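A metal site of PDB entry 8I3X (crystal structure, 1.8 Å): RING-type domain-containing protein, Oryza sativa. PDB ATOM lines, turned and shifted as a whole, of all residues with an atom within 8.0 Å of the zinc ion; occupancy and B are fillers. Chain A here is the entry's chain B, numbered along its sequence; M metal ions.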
ATOM      1  N   SER A  13      20.160 -13.562 -15.434  1.00  0.00           N
ATOM      2  CA  SER A  13      20.567 -13.003 -16.716  1.00  0.00           C
ATOM      3  C   SER A  13      22.050 -13.261 -16.978  1.00  0.00           C
ATOM      4  O   SER A  13      22.866 -13.289 -16.059  1.00  0.00           O
ATOM      5  CB  SER A  13      20.272 -11.501 -16.773  1.00  0.00           C
ATOM      6  OG  SER A  13      21.124 -10.779 -15.916  1.00  0.00           O
ATOM      7  N   CYS A  14      22.378 -13.454 -18.258  1.00  0.00           N
ATOM      8  CA  CYS A  14      23.751 -13.666 -18.671  1.00  0.00           C
ATOM      9  C   CYS A  14      24.474 -12.321 -18.711  1.00  0.00           C
ATOM     10  O   CYS A  14      24.097 -11.429 -19.474  1.00  0.00           O
ATOM     11  CB  CYS A  14      23.780 -14.345 -20.043  1.00  0.00           C
ATOM     12  SG  CYS A  14      25.423 -14.571 -20.789  1.00  0.00           S
ATOM     13  N   SER A  15      25.513 -12.169 -17.895  1.00  0.00           N
ATOM     14  CA  SER A  15      26.249 -10.909 -17.856  1.00  0.00           C
ATOM     15  C   SER A  15      26.985 -10.606 -19.150  1.00  0.00           C
ATOM     16  O   SER A  15      27.465  -9.481 -19.324  1.00  0.00           O
ATOM     17  CB  SER A  15      27.250 -10.924 -16.700  1.00  0.00           C
ATOM     18  OG  SER A  15      28.400 -11.680 -17.053  1.00  0.00           O
ATOM     19  N   ILE A  16      27.091 -11.578 -20.057  1.00  0.00           N
ATOM     20  CA  ILE A  16      27.860 -11.372 -21.280  1.00  0.00           C
ATOM     21  C   ILE A  16      27.016 -10.691 -22.339  1.00  0.00           C
ATOM     22  O   ILE A  16      27.435  -9.715 -22.970  1.00  0.00           O
ATOM     23  CB  ILE A  16      28.433 -12.710 -21.761  1.00  0.00           C
ATOM     24  CG1 ILE A  16      29.442 -13.248 -20.743  1.00  0.00           C
ATOM     25  CG2 ILE A  16      29.058 -12.553 -23.128  1.00  0.00           C
ATOM     26  CD1 ILE A  16      30.057 -14.564 -21.101  1.00  0.00           C
ATOM     27  N   CYS A  17      25.810 -11.189 -22.563  1.00  0.00           N
ATOM     28  CA  CYS A  17      24.912 -10.635 -23.559  1.00  0.00           C
ATOM     29  C   CYS A  17      23.736  -9.902 -22.940  1.00  0.00           C
ATOM     30  O   CYS A  17      22.935  -9.306 -23.676  1.00  0.00           O
ATOM     31  CB  CYS A  17      24.412 -11.741 -24.486  1.00  0.00           C
ATOM     32  SG  CYS A  17      23.261 -12.898 -23.690  1.00  0.00           S
ATOM     33  N   LEU A  18      23.606  -9.955 -21.610  1.00  0.00           N
ATOM     34  CA  LEU A  18      22.556  -9.271 -20.843  1.00  0.00           C
ATOM     35  C   LEU A  18      21.165  -9.816 -21.124  1.00  0.00           C
ATOM     36  O   LEU A  18      20.169  -9.171 -20.798  1.00  0.00           O
ATOM     37  CB  LEU A  18      22.601  -7.754 -21.064  1.00  0.00           C
ATOM     38  CG  LEU A  18      23.714  -7.036 -20.296  1.00  0.00           C
ATOM     39  CD1 LEU A  18      23.823  -7.595 -18.883  1.00  0.00           C
ATOM     40  CD2 LEU A  18      25.055  -7.145 -20.996  1.00  0.00           C
ATOM     41  N   ASP A  19      21.063 -11.007 -21.710  1.00  0.00           N
ATOM     42  CA  ASP A  19      19.787 -11.678 -21.925  1.00  0.00           C
ATOM     43  C   ASP A  19      19.534 -12.700 -20.825  1.00  0.00           C
ATOM     44  O   ASP A  19      20.458 -13.193 -20.170  1.00  0.00           O
ATOM     45  CB  ASP A  19      19.734 -12.358 -23.286  1.00  0.00           C
ATOM     46  CG  ASP A  19      19.558 -11.382 -24.416  1.00  0.00           C
ATOM     47  OD1 ASP A  19      19.373 -10.178 -24.132  1.00  0.00           O
ATOM     48  OD2 ASP A  19      19.613 -11.817 -25.588  1.00  0.00           O
ATOM     49  N   ALA A  20      18.264 -13.032 -20.634  1.00  0.00           N
ATOM     50  CA  ALA A  20      17.901 -13.996 -19.609  1.00  0.00           C
ATOM     51  C   ALA A  20      18.419 -15.383 -19.976  1.00  0.00           C
ATOM     52  O   ALA A  20      18.345 -15.815 -21.132  1.00  0.00           O
ATOM     53  CB  ALA A  20      16.384 -14.042 -19.425  1.00  0.00           C
ATOM     54  N   VAL A  21      18.973 -16.063 -18.972  1.00  0.00           N
ATOM     55  CA  VAL A  21      19.341 -17.469 -19.093  1.00  0.00           C
ATOM     56  C   VAL A  21      18.126 -18.295 -18.660  1.00  0.00           C
ATOM     57  O   VAL A  21      17.668 -18.168 -17.528  1.00  0.00           O
ATOM     58  CB  VAL A  21      20.559 -17.800 -18.226  1.00  0.00           C
ATOM     59  CG1 VAL A  21      20.888 -19.278 -18.299  1.00  0.00           C
ATOM     60  CG2 VAL A  21      21.745 -16.946 -18.622  1.00  0.00           C
ATOM     61  N   ARG A  28      18.058 -21.709 -26.030  1.00  0.00           N
ATOM     62  CA  ARG A  28      19.500 -21.590 -26.105  1.00  0.00           C
ATOM     63  C   ARG A  28      20.128 -22.457 -25.024  1.00  0.00           C
ATOM     64  O   ARG A  28      19.588 -22.550 -23.913  1.00  0.00           O
ATOM     65  CB  ARG A  28      19.967 -20.129 -25.899  1.00  0.00           C
ATOM     66  CG  ARG A  28      19.716 -19.185 -27.064  1.00  0.00           C
ATOM     67  CD  ARG A  28      20.124 -17.765 -26.679  1.00  0.00           C
ATOM     68  NE  ARG A  28      21.579 -17.586 -26.665  1.00  0.00           N
ATOM     69  CZ  ARG A  28      22.196 -16.473 -26.286  1.00  0.00           C
ATOM     70  NH1 ARG A  28      21.489 -15.427 -25.880  1.00  0.00           N
ATOM     71  NH2 ARG A  28      23.523 -16.414 -26.319  1.00  0.00           N
ATOM     72  N   SER A  29      21.256 -23.078 -25.347  1.00  0.00           N
ATOM     73  CA  SER A  29      21.946 -23.900 -24.374  1.00  0.00           C
ATOM     74  C   SER A  29      22.501 -23.031 -23.249  1.00  0.00           C
ATOM     75  O   SER A  29      22.783 -21.836 -23.436  1.00  0.00           O
ATOM     76  CB  SER A  29      23.083 -24.681 -25.039  1.00  0.00           C
ATOM     77  OG  SER A  29      22.557 -25.530 -26.043  1.00  0.00           O
ATOM     78  N   GLU A  38      25.741 -18.199 -13.970  1.00  0.00           N
ATOM     79  CA  GLU A  38      25.149 -18.854 -15.116  1.00  0.00           C
ATOM     80  C   GLU A  38      25.212 -17.978 -16.354  1.00  0.00           C
ATOM     81  O   GLU A  38      25.206 -16.747 -16.271  1.00  0.00           O
ATOM     82  CB  GLU A  38      23.692 -19.230 -14.836  1.00  0.00           C
ATOM     83  CG  GLU A  38      23.525 -20.102 -13.608  1.00  0.00           C
ATOM     84  CD  GLU A  38      22.069 -20.384 -13.318  1.00  0.00           C
ATOM     85  OE1 GLU A  38      21.382 -20.920 -14.204  1.00  0.00           O
ATOM     86  OE2 GLU A  38      21.621 -20.062 -12.186  1.00  0.00           O
ATOM     87  N   PHE A  39      25.262 -18.638 -17.496  1.00  0.00           N
ATOM     88  CA  PHE A  39      25.505 -18.002 -18.780  1.00  0.00           C
ATOM     89  C   PHE A  39      24.843 -18.831 -19.858  1.00  0.00           C
ATOM     90  O   PHE A  39      24.531 -20.005 -19.664  1.00  0.00           O
ATOM     91  CB  PHE A  39      27.002 -17.883 -19.068  1.00  0.00           C
ATOM     92  CG  PHE A  39      27.784 -17.187 -17.988  1.00  0.00           C
ATOM     93  CD1 PHE A  39      27.918 -15.806 -17.989  1.00  0.00           C
ATOM     94  CD2 PHE A  39      28.386 -17.908 -16.971  1.00  0.00           C
ATOM     95  CE1 PHE A  39      28.633 -15.163 -17.000  1.00  0.00           C
ATOM     96  CE2 PHE A  39      29.094 -17.271 -15.977  1.00  0.00           C
ATOM     97  CZ  PHE A  39      29.224 -15.896 -15.991  1.00  0.00           C
ATOM     98  N   HIS A  40      24.645 -18.220 -21.022  1.00  0.00           N
ATOM     99  CA  HIS A  40      24.392 -19.023 -22.202  1.00  0.00           C
ATOM    100  C   HIS A  40      25.668 -19.758 -22.589  1.00  0.00           C
ATOM    101  O   HIS A  40      26.779 -19.258 -22.385  1.00  0.00           O
ATOM    102  CB  HIS A  40      23.918 -18.154 -23.365  1.00  0.00           C
ATOM    103  CG  HIS A  40      22.700 -17.359 -23.034  1.00  0.00           C
ATOM    104  ND1 HIS A  40      22.747 -16.016 -22.727  1.00  0.00           N
ATOM    105  CD2 HIS A  40      21.401 -17.726 -22.941  1.00  0.00           C
ATOM    106  CE1 HIS A  40      21.521 -15.597 -22.463  1.00  0.00           C
ATOM    107  NE2 HIS A  40      20.689 -16.612 -22.583  1.00  0.00           N
ATOM    108  N   LEU A  41      25.511 -20.958 -23.136  1.00  0.00           N
ATOM    109  CA  LEU A  41      26.682 -21.771 -23.469  1.00  0.00           C
ATOM    110  C   LEU A  41      27.599 -21.061 -24.471  1.00  0.00           C
ATOM    111  O   LEU A  41      28.821 -21.040 -24.279  1.00  0.00           O
ATOM    112  CB  LEU A  41      26.265 -23.133 -24.001  1.00  0.00           C
ATOM    113  CG  LEU A  41      27.444 -24.065 -24.301  1.00  0.00           C
ATOM    114  CD1 LEU A  41      28.362 -24.170 -23.115  1.00  0.00           C
ATOM    115  CD2 LEU A  41      26.897 -25.443 -24.678  1.00  0.00           C
ATOM    116  N   ASP A  42      27.048 -20.489 -25.536  1.00  0.00           N
ATOM    117  CA  ASP A  42      27.947 -19.898 -26.540  1.00  0.00           C
ATOM    118  C   ASP A  42      28.608 -18.633 -26.004  1.00  0.00           C
ATOM    119  O   ASP A  42      29.751 -18.338 -26.365  1.00  0.00           O
ATOM    120  CB  ASP A  42      27.214 -19.661 -27.875  1.00  0.00           C
ATOM    121  CG  ASP A  42      25.981 -18.762 -27.745  1.00  0.00           C
ATOM    122  OD1 ASP A  42      25.626 -18.346 -26.624  1.00  0.00           O
ATOM    123  OD2 ASP A  42      25.366 -18.488 -28.800  1.00  0.00           O
ATOM    124  N   CYS A  43      27.926 -17.882 -25.141  1.00  0.00           N
ATOM    125  CA  CYS A  43      28.553 -16.719 -24.528  1.00  0.00           C
ATOM    126  C   CYS A  43      29.778 -17.101 -23.713  1.00  0.00           C
ATOM    127  O   CYS A  43      30.887 -16.597 -23.953  1.00  0.00           O
ATOM    128  CB  CYS A  43      27.535 -16.003 -23.640  1.00  0.00           C
ATOM    129  SG  CYS A  43      26.269 -15.206 -24.589  1.00  0.00           S
ATOM    130  N   ILE A  44      29.597 -17.978 -22.731  1.00  0.00           N
ATOM    131  CA  ILE A  44      30.706 -18.290 -21.823  1.00  0.00           C
ATOM    132  C   ILE A  44      31.777 -19.097 -22.544  1.00  0.00           C
ATOM    133  O   ILE A  44      32.977 -18.942 -22.264  1.00  0.00           O
ATOM    134  CB  ILE A  44      30.187 -19.018 -20.562  1.00  0.00           C
ATOM    135  CG1 ILE A  44      31.248 -19.032 -19.466  1.00  0.00           C
ATOM    136  CG2 ILE A  44      29.743 -20.423 -20.876  1.00  0.00           C
ATOM    137  CD1 ILE A  44      31.573 -17.661 -18.925  1.00  0.00           C
HETATM  138 ZN    ZN M   1      24.574 -14.698 -22.990  1.00  0.00          ZN
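ND1 of His 40 lies close to NH1 of Arg 28 (3.4 Å).
A ring nitrogen (NE2) of His 40 lies within hydrogen-bond range of the backbone carbonyl oxygen (O) of Ala 20 (2.9 Å).
The side-chain sulfur (SG) of Cys 17 sits close to the guanidinium group (NH1) of Arg 28.
N of Ile 16 lies close to SG of Cys 14 (3.5 Å).
N of Cys 14 is in hydrogen-bond range of O of Asp 19 (2.7 Å).
The guanidinium group (NH2) of Arg 28 sits close to the side-chain sulfur (SG) of Cys 43 (3.5 Å).
The side-chain carboxylate (OD1) of Asp 42 sits close to the side-chain sulfur (SG) of Cys 43 (3.8 Å).
The guanidinium group (NH2) of Arg 28 is in salt-bridge range of the side-chain carboxylate (OD1) of Asp 42.
A ring nitrogen (ND1) of His 40 is bound to the zinc ion (2.3 Å).
SG of Cys 17 is bound to the zinc ion.
The zinc ion is bound by the side-chain sulfur (SG) of Cys 14 (2.4 Å).
The zinc ion is bound by SG of Cys 43, at 2.4 Å.
Arg 28 touches the zinc ion (NH2 to ZN, 3.9 Å).
Five residues have an atom within 4 Å of the zinc ion: Cys 14, Cys 17, Arg 28, His 40 and Cys 43.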
